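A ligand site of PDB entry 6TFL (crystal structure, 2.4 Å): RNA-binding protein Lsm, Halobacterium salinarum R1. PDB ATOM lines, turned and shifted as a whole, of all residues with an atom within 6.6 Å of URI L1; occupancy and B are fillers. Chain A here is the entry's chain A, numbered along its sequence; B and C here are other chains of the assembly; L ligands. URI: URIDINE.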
ATOM      1  N   ASP A  37       4.706   2.188  -6.901  1.00  0.00           N
ATOM      2  CA  ASP A  37       5.943   2.700  -6.319  1.00  0.00           C
ATOM      3  C   ASP A  37       6.654   3.619  -7.312  1.00  0.00           C
ATOM      4  O   ASP A  37       6.195   3.836  -8.433  1.00  0.00           O
ATOM      5  CB  ASP A  37       6.839   1.549  -5.845  1.00  0.00           C
ATOM      6  CG  ASP A  37       7.280   0.645  -6.984  1.00  0.00           C
ATOM      7  OD1 ASP A  37       7.471   1.122  -8.137  1.00  0.00           O
ATOM      8  OD2 ASP A  37       7.454  -0.576  -6.703  1.00  0.00           O
ATOM      9  N   GLN A  38       7.808   4.130  -6.886  1.00  0.00           N
ATOM     10  CA  GLN A  38       8.591   5.094  -7.659  1.00  0.00           C
ATOM     11  C   GLN A  38       9.012   4.583  -9.026  1.00  0.00           C
ATOM     12  O   GLN A  38       9.292   5.398  -9.900  1.00  0.00           O
ATOM     13  CB  GLN A  38       9.829   5.494  -6.863  1.00  0.00           C
ATOM     14  CG  GLN A  38       9.612   5.424  -5.339  1.00  0.00           C
ATOM     15  CD  GLN A  38       9.848   4.016  -4.756  1.00  0.00           C
ATOM     16  OE1 GLN A  38      10.734   3.285  -5.201  1.00  0.00           O
ATOM     17  NE2 GLN A  38       9.029   3.652  -3.765  1.00  0.00           N
ATOM     18  N   HIS A  39       9.101   3.278  -9.224  1.00  0.00           N
ATOM     19  CA  HIS A  39       9.424   2.781 -10.566  1.00  0.00           C
ATOM     20  C   HIS A  39       8.208   2.691 -11.471  1.00  0.00           C
ATOM     21  O   HIS A  39       8.346   2.307 -12.633  1.00  0.00           O
ATOM     22  CB  HIS A  39      10.058   1.391 -10.493  1.00  0.00           C
ATOM     23  CG  HIS A  39      11.156   1.277  -9.507  1.00  0.00           C
ATOM     24  ND1 HIS A  39      12.395   1.857  -9.697  1.00  0.00           N
ATOM     25  CD2 HIS A  39      11.221   0.629  -8.318  1.00  0.00           C
ATOM     26  CE1 HIS A  39      13.173   1.583  -8.660  1.00  0.00           C
ATOM     27  NE2 HIS A  39      12.481   0.839  -7.807  1.00  0.00           N
ATOM     28  N   MET A  40       7.024   3.021 -10.952  1.00  0.00           N
ATOM     29  CA  MET A  40       5.754   2.802 -11.611  1.00  0.00           C
ATOM     30  C   MET A  40       5.426   1.321 -11.745  1.00  0.00           C
ATOM     31  O   MET A  40       4.657   0.943 -12.640  1.00  0.00           O
ATOM     32  CB  MET A  40       5.671   3.494 -12.979  1.00  0.00           C
ATOM     33  CG  MET A  40       4.369   4.235 -13.199  1.00  0.00           C
ATOM     34  SD  MET A  40       4.196   4.988 -14.849  1.00  0.00           S
ATOM     35  CE  MET A  40       4.916   6.599 -14.536  1.00  0.00           C
ATOM     36  N   ASN A  41       5.987   0.464 -10.881  1.00  0.00           N
ATOM     37  CA  ASN A  41       5.332  -0.805 -10.608  1.00  0.00           C
ATOM     38  C   ASN A  41       3.932  -0.491 -10.080  1.00  0.00           C
ATOM     39  O   ASN A  41       3.773   0.425  -9.268  1.00  0.00           O
ATOM     40  CB  ASN A  41       6.083  -1.628  -9.570  1.00  0.00           C
ATOM     41  CG  ASN A  41       7.557  -1.851  -9.901  1.00  0.00           C
ATOM     42  OD1 ASN A  41       7.966  -1.879 -11.070  1.00  0.00           O
ATOM     43  ND2 ASN A  41       8.368  -2.056  -8.864  1.00  0.00           N
ATOM     44  N   ARG A  53       5.380  -4.985 -13.353  1.00  0.00           N
ATOM     45  CA  ARG A  53       6.653  -4.278 -13.242  1.00  0.00           C
ATOM     46  C   ARG A  53       6.635  -3.078 -14.178  1.00  0.00           C
ATOM     47  O   ARG A  53       6.246  -3.190 -15.350  1.00  0.00           O
ATOM     48  CB  ARG A  53       7.815  -5.220 -13.557  1.00  0.00           C
ATOM     49  CG  ARG A  53       9.085  -4.869 -12.806  1.00  0.00           C
ATOM     50  CD  ARG A  53      10.241  -5.749 -13.247  1.00  0.00           C
ATOM     51  NE  ARG A  53      11.518  -5.352 -12.650  1.00  0.00           N
ATOM     52  CZ  ARG A  53      12.502  -4.784 -13.335  1.00  0.00           C
ATOM     53  NH1 ARG A  53      13.641  -4.460 -12.720  1.00  0.00           N
ATOM     54  NH2 ARG A  53      12.360  -4.534 -14.632  1.00  0.00           N
ATOM     55  N   GLY A  54       7.048  -1.918 -13.649  1.00  0.00           N
ATOM     56  CA  GLY A  54       6.885  -0.665 -14.356  1.00  0.00           C
ATOM     57  C   GLY A  54       7.566  -0.624 -15.718  1.00  0.00           C
ATOM     58  O   GLY A  54       7.066   0.019 -16.646  1.00  0.00           O
ATOM     59  N   ASP A  55       8.704  -1.310 -15.862  1.00  0.00           N
ATOM     60  CA  ASP A  55       9.451  -1.241 -17.110  1.00  0.00           C
ATOM     61  C   ASP A  55       8.636  -1.719 -18.305  1.00  0.00           C
ATOM     62  O   ASP A  55       8.980  -1.368 -19.434  1.00  0.00           O
ATOM     63  CB  ASP A  55      10.754  -2.039 -16.994  1.00  0.00           C
ATOM     64  CG  ASP A  55      10.535  -3.548 -17.106  1.00  0.00           C
ATOM     65  OD1 ASP A  55      11.105  -4.154 -18.040  1.00  0.00           O
ATOM     66  OD2 ASP A  55       9.831  -4.133 -16.235  1.00  0.00           O
ATOM     67  N   ASN A  56       7.571  -2.488 -18.099  1.00  0.00           N
ATOM     68  CA  ASN A  56       6.695  -2.932 -19.191  1.00  0.00           C
ATOM     69  C   ASN A  56       5.583  -1.946 -19.537  1.00  0.00           C
ATOM     70  O   ASN A  56       4.879  -2.153 -20.528  1.00  0.00           O
ATOM     71  CB  ASN A  56       6.056  -4.277 -18.842  1.00  0.00           C
ATOM     72  CG  ASN A  56       7.071  -5.311 -18.389  1.00  0.00           C
ATOM     73  OD1 ASN A  56       7.799  -5.866 -19.208  1.00  0.00           O
ATOM     74  ND2 ASN A  56       7.140  -5.565 -17.074  1.00  0.00           N
ATOM     75  N   ARG B  53       4.577   6.654 -19.632  1.00  0.00           N
ATOM     76  CA  ARG B  53       5.876   6.421 -19.026  1.00  0.00           C
ATOM     77  C   ARG B  53       6.972   6.937 -19.964  1.00  0.00           C
ATOM     78  O   ARG B  53       6.975   6.644 -21.164  1.00  0.00           O
ATOM     79  CB  ARG B  53       6.033   4.939 -18.722  1.00  0.00           C
ATOM     80  CG  ARG B  53       7.090   4.676 -17.684  1.00  0.00           C
ATOM     81  CD  ARG B  53       7.010   3.285 -17.134  1.00  0.00           C
ATOM     82  NE  ARG B  53       8.050   3.054 -16.148  1.00  0.00           N
ATOM     83  CZ  ARG B  53       9.290   2.689 -16.462  1.00  0.00           C
ATOM     84  NH1 ARG B  53       9.603   2.502 -17.738  1.00  0.00           N
ATOM     85  NH2 ARG B  53      10.178   2.489 -15.498  1.00  0.00           N
ATOM     86  N   ASP B  55      10.076   6.386 -20.703  1.00  0.00           N
ATOM     87  CA  ASP B  55      10.956   5.590 -21.552  1.00  0.00           C
ATOM     88  C   ASP B  55      10.292   5.171 -22.870  1.00  0.00           C
ATOM     89  O   ASP B  55      10.986   4.620 -23.721  1.00  0.00           O
ATOM     90  CB  ASP B  55      11.488   4.375 -20.775  1.00  0.00           C
ATOM     91  CG  ASP B  55      10.564   3.159 -20.847  1.00  0.00           C
ATOM     92  OD1 ASP B  55      11.100   2.037 -20.896  1.00  0.00           O
ATOM     93  OD2 ASP B  55       9.336   3.308 -20.829  1.00  0.00           O
ATOM     94  N   LEU C   8       6.199  -4.049  -3.767  1.00  0.00           N
ATOM     95  CA  LEU C   8       7.117  -4.878  -3.002  1.00  0.00           C
ATOM     96  C   LEU C   8       6.484  -5.344  -1.691  1.00  0.00           C
ATOM     97  O   LEU C   8       6.805  -6.443  -1.217  1.00  0.00           O
ATOM     98  CB  LEU C   8       8.417  -4.115  -2.733  1.00  0.00           C
ATOM     99  CG  LEU C   8       9.296  -3.805  -3.956  1.00  0.00           C
ATOM    100  CD1 LEU C   8      10.741  -3.573  -3.541  1.00  0.00           C
ATOM    101  CD2 LEU C   8       9.213  -4.910  -4.969  1.00  0.00           C
ATOM    102  N   ASP C  37      13.980  -9.258  -3.995  1.00  0.00           N
ATOM    103  CA  ASP C  37      14.731  -8.071  -3.622  1.00  0.00           C
ATOM    104  C   ASP C  37      14.124  -6.833  -4.291  1.00  0.00           C
ATOM    105  O   ASP C  37      13.100  -6.905  -4.964  1.00  0.00           O
ATOM    106  CB  ASP C  37      16.221  -8.218  -3.929  1.00  0.00           C
ATOM    107  CG  ASP C  37      16.527  -8.483  -5.407  1.00  0.00           C
ATOM    108  OD1 ASP C  37      15.725  -8.101  -6.307  1.00  0.00           O
ATOM    109  OD2 ASP C  37      17.591  -9.095  -5.650  1.00  0.00           O
ATOM    110  N   GLN C  38      14.785  -5.692  -4.095  1.00  0.00           N
ATOM    111  CA  GLN C  38      14.337  -4.399  -4.559  1.00  0.00           C
ATOM    112  C   GLN C  38      14.381  -4.242  -6.081  1.00  0.00           C
ATOM    113  O   GLN C  38      13.809  -3.280  -6.612  1.00  0.00           O
ATOM    114  CB  GLN C  38      15.182  -3.320  -3.903  1.00  0.00           C
ATOM    115  CG  GLN C  38      16.571  -3.203  -4.521  1.00  0.00           C
ATOM    116  CD  GLN C  38      17.699  -3.691  -3.606  1.00  0.00           C
ATOM    117  OE1 GLN C  38      17.559  -4.683  -2.864  1.00  0.00           O
ATOM    118  NE2 GLN C  38      18.836  -3.013  -3.676  1.00  0.00           N
ATOM    119  N   HIS C  39      15.055  -5.133  -6.813  1.00  0.00           N
ATOM    120  CA  HIS C  39      14.976  -5.126  -8.264  1.00  0.00           C
ATOM    121  C   HIS C  39      13.796  -5.915  -8.773  1.00  0.00           C
ATOM    122  O   HIS C  39      13.582  -5.990  -9.989  1.00  0.00           O
ATOM    123  CB  HIS C  39      16.259  -5.703  -8.882  1.00  0.00           C
ATOM    124  CG  HIS C  39      17.508  -5.001  -8.444  1.00  0.00           C
ATOM    125  ND1 HIS C  39      17.846  -3.740  -8.871  1.00  0.00           N
ATOM    126  CD2 HIS C  39      18.494  -5.382  -7.594  1.00  0.00           C
ATOM    127  CE1 HIS C  39      18.981  -3.371  -8.324  1.00  0.00           C
ATOM    128  NE2 HIS C  39      19.399  -4.348  -7.540  1.00  0.00           N
ATOM    129  N   MET C  40      13.038  -6.523  -7.859  1.00  0.00           N
ATOM    130  CA  MET C  40      12.042  -7.541  -8.172  1.00  0.00           C
ATOM    131  C   MET C  40      12.689  -8.809  -8.748  1.00  0.00           C
ATOM    132  O   MET C  40      12.042  -9.569  -9.473  1.00  0.00           O
ATOM    133  CB  MET C  40      10.946  -7.013  -9.101  1.00  0.00           C
ATOM    134  CG  MET C  40       9.576  -7.678  -8.898  1.00  0.00           C
ATOM    135  SD  MET C  40       8.155  -6.768  -9.582  1.00  0.00           S
ATOM    136  CE  MET C  40       8.118  -5.349  -8.473  1.00  0.00           C
ATOM    137  N   ASN C  41      13.957  -9.070  -8.408  1.00  0.00           N
ATOM    138  CA  ASN C  41      14.433 -10.441  -8.473  1.00  0.00           C
ATOM    139  C   ASN C  41      13.598 -11.275  -7.511  1.00  0.00           C
ATOM    140  O   ASN C  41      13.197 -10.786  -6.439  1.00  0.00           O
ATOM    141  CB  ASN C  41      15.912 -10.541  -8.122  1.00  0.00           C
ATOM    142  CG  ASN C  41      16.818  -9.703  -9.025  1.00  0.00           C
ATOM    143  OD1 ASN C  41      16.600  -9.594 -10.234  1.00  0.00           O
ATOM    144  ND2 ASN C  41      17.879  -9.154  -8.431  1.00  0.00           N
ATOM    145  N   ASP C  55      14.343  -7.984 -14.325  1.00  0.00           N
ATOM    146  CA  ASP C  55      14.087  -7.283 -15.572  1.00  0.00           C
ATOM    147  C   ASP C  55      13.479  -8.181 -16.657  1.00  0.00           C
ATOM    148  O   ASP C  55      13.096  -7.656 -17.702  1.00  0.00           O
ATOM    149  CB  ASP C  55      15.367  -6.620 -16.075  1.00  0.00           C
ATOM    150  CG  ASP C  55      16.237  -7.561 -16.880  1.00  0.00           C
ATOM    151  OD1 ASP C  55      16.872  -8.450 -16.282  1.00  0.00           O
ATOM    152  OD2 ASP C  55      16.296  -7.399 -18.125  1.00  0.00           O
HETATM  153  N1  URI L   1      12.639  -1.105 -12.189  1.00  0.00           N
HETATM  154  C2  URI L   1      11.318  -1.529 -12.216  1.00  0.00           C
HETATM  155  N3  URI L   1      10.909  -2.237 -11.119  1.00  0.00           N
HETATM  156  C4  URI L   1      11.661  -2.555 -10.015  1.00  0.00           C
HETATM  157  C5  URI L   1      13.006  -2.066 -10.046  1.00  0.00           C
HETATM  158  C6  URI L   1      13.439  -1.364 -11.101  1.00  0.00           C
HETATM  159  O2  URI L   1      10.568  -1.301 -13.152  1.00  0.00           O
HETATM  160  O4  URI L   1      11.111  -3.200  -9.114  1.00  0.00           O
HETATM  161  C1' URI L   1      13.053  -0.319 -13.359  1.00  0.00           C
HETATM  162  C2' URI L   1      12.963   1.183 -13.159  1.00  0.00           C
HETATM  163  C3' URI L   1      13.872   1.677 -14.275  1.00  0.00           C
HETATM  164  C4' URI L   1      14.986   0.631 -14.276  1.00  0.00           C
HETATM  165  O2' URI L   1      11.636   1.650 -13.219  1.00  0.00           O
HETATM  166  O3' URI L   1      13.172   1.644 -15.517  1.00  0.00           O
HETATM  167  O4' URI L   1      14.412  -0.575 -13.676  1.00  0.00           O
HETATM  168  C5' URI L   1      16.232   1.041 -13.532  1.00  0.00           C
HETATM  169  O5' URI L   1      16.809   2.235 -14.083  1.00  0.00           O
HETATM  170  N1  URI L   2      18.611  -5.378 -12.197  1.00  0.00           N
HETATM  171  C2  URI L   2      17.954  -6.584 -12.005  1.00  0.00           C
HETATM  172  N3  URI L   2      18.604  -7.456 -11.157  1.00  0.00           N
HETATM  173  C4  URI L   2      19.795  -7.250 -10.506  1.00  0.00           C
HETATM  174  C5  URI L   2      20.412  -5.982 -10.748  1.00  0.00           C
HETATM  175  C6  URI L   2      19.809  -5.105 -11.571  1.00  0.00           C
HETATM  176  O2  URI L   2      16.887  -6.879 -12.539  1.00  0.00           O
HETATM  177  O4  URI L   2      20.238  -8.129  -9.776  1.00  0.00           O
HETATM  178  C1' URI L   2      17.979  -4.397 -13.094  1.00  0.00           C
HETATM  179  C2' URI L   2      17.226  -3.290 -12.364  1.00  0.00           C
HETATM  180  C3' URI L   2      17.181  -2.216 -13.458  1.00  0.00           C
HETATM  181  C4' URI L   2      18.563  -2.346 -14.090  1.00  0.00           C
HETATM  182  O2' URI L   2      15.975  -3.728 -11.868  1.00  0.00           O
HETATM  183  O3' URI L   2      16.187  -2.542 -14.433  1.00  0.00           O
HETATM  184  O4' URI L   2      18.976  -3.729 -13.854  1.00  0.00           O
HETATM  185  C5' URI L   2      19.588  -1.398 -13.522  1.00  0.00           C
HETATM  186  O5' URI L   2      19.332  -0.042 -13.876  1.00  0.00           O
HETATM  187  N1  URI L   3      12.078   5.461 -16.251  1.00  0.00           N
HETATM  188  C2  URI L   3      12.195   5.118 -14.909  1.00  0.00           C
HETATM  189  N3  URI L   3      11.059   5.309 -14.156  1.00  0.00           N
HETATM  190  C4  URI L   3       9.846   5.802 -14.564  1.00  0.00           C
HETATM  191  C5  URI L   3       9.799   6.153 -15.955  1.00  0.00           C
HETATM  192  C6  URI L   3      10.888   5.985 -16.721  1.00  0.00           C
HETATM  193  O2  URI L   3      13.201   4.662 -14.390  1.00  0.00           O
HETATM  194  O4  URI L   3       8.925   5.915 -13.742  1.00  0.00           O
HETATM  195  C1' URI L   3      13.212   5.344 -17.212  1.00  0.00           C
HETATM  196  C2' URI L   3      14.565   5.877 -16.694  1.00  0.00           C
HETATM  197  C3' URI L   3      15.386   4.591 -16.570  1.00  0.00           C
HETATM  198  C4' URI L   3      14.813   3.714 -17.677  1.00  0.00           C
HETATM  199  O2' URI L   3      15.131   6.710 -17.686  1.00  0.00           O
HETATM  200  O3' URI L   3      16.780   4.815 -16.721  1.00  0.00           O
HETATM  201  O4' URI L   3      13.390   4.001 -17.624  1.00  0.00           O
HETATM  202  C5' URI L   3      15.108   2.235 -17.642  1.00  0.00           C
HETATM  203  O5' URI L   3      16.163   1.907 -18.537  1.00  0.00           O
HETATM  204  N1  URI L   4      16.817   9.400 -19.716  1.00  0.00           N
HETATM  205  C2  URI L   4      16.553  10.268 -20.766  1.00  0.00           C
HETATM  206  N3  URI L   4      15.737  11.323 -20.424  1.00  0.00           N
HETATM  207  C4  URI L   4      15.188  11.582 -19.186  1.00  0.00           C
HETATM  208  C5  URI L   4      15.530  10.637 -18.158  1.00  0.00           C
HETATM  209  C6  URI L   4      16.318   9.607 -18.456  1.00  0.00           C
HETATM  210  O2  URI L   4      16.989  10.116 -21.914  1.00  0.00           O
HETATM  211  O4  URI L   4      14.466  12.578 -19.044  1.00  0.00           O
HETATM  212  C1' URI L   4      17.711   8.276 -20.022  1.00  0.00           C
HETATM  213  C2' URI L   4      18.326   7.588 -18.815  1.00  0.00           C
HETATM  214  C3' URI L   4      18.745   6.249 -19.428  1.00  0.00           C
HETATM  215  C4' URI L   4      17.639   5.987 -20.453  1.00  0.00           C
HETATM  216  O2' URI L   4      19.400   8.340 -18.292  1.00  0.00           O
HETATM  217  O3' URI L   4      19.959   6.453 -20.142  1.00  0.00           O
HETATM  218  O4' URI L   4      16.994   7.274 -20.695  1.00  0.00           O
HETATM  219  C5' URI L   4      16.605   4.979 -20.059  1.00  0.00           C
HETATM  220  O5' URI L   4      15.361   5.202 -20.712  1.00  0.00           O
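The guanidinium group (NH2) of Arg 53 of chain B lies within hydrogen-bond range of an oxygen (O2') of URI L1 (2.8 Å). OD1 of Asn 41 of chain A is in hydrogen-bond range of N3 of URI L1, 3.0 Å away. The backbone carbonyl oxygen (O) of His 39 of chain A lies close to an oxygen (O2') of URI L1 (3.4 Å). N of Asp 55 of chain A sits at hydrogen-bond distance from O2 of URI L1, at 3.3 Å. The guanidinium group (NH1) of Arg 53 of chain A is in hydrogen-bond range of an oxygen (O2') of URI L2, at 2.6 Å. ND2 of Asn 41 of chain C sits at hydrogen-bond distance from O4 of URI L2 (2.9 Å). N of Asp 55 of chain C sits at hydrogen-bond distance from O2 of URI L2 (3.3 Å).
O3' of URI L2 sits at hydrogen-bond distance from O4' of URI L1, at 2.8 Å. An oxygen (O4') of URI L3 lies close to an oxygen (O3') of URI L1, at 3.2 Å. O2' of URI L3 lies close to O5' of URI L4, at 3.4 Å.
The guanidinium group (NH2) of Arg 53 of chain B lies within hydrogen-bond range of the backbone carbonyl oxygen (O) of His 39 of chain A (3.4 Å). NH1 of Arg 53 of chain B is in salt-bridge range of OD2 of Asp 55 of chain B, at 3.2 Å. The side-chain amide oxygen (OD1) of Asn 41 of chain A sits at hydrogen-bond distance from the backbone NH (N) of Gly 54 (2.7 Å). OD2 of Asp 37 of chain A lies within hydrogen-bond range of ND2 of Asn 41 of chain A, at 2.8 Å. OD1 of Asp 37 of chain A sits at hydrogen-bond distance from N of His 39 of chain A. The backbone carbonyl oxygen of His 39 of chain C is in hydrogen-bond range of the guanidinium group of Arg 53 of chain A. The backbone carbonyl oxygen of Arg 53 of chain A lies within hydrogen-bond range of the side-chain amide nitrogen of Asn 56 (3.1 Å). OD1 of Asp 37 of chain C lies within hydrogen-bond range of N of His 39 of chain C, at 3.1 Å.
Arg 53 of chain A touches URI L1 (NH1 to C6, 3.5 Å). Gly 54 touches URI L1. O of Gln 38 of chain C touches O4 of URI L1 (3.7 Å). His 39 of chain C touches URI L1 (O to O4, 3.8 Å). Met 40 of chain C touches URI L1 (CE to O4, 3.7 Å). Hydrophobic or aromatic side chains that line URI L1: His 39 of chain A and Met 40 of chain C. Of the 18 residues printed, 9 come within 4 Å of URI L1.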
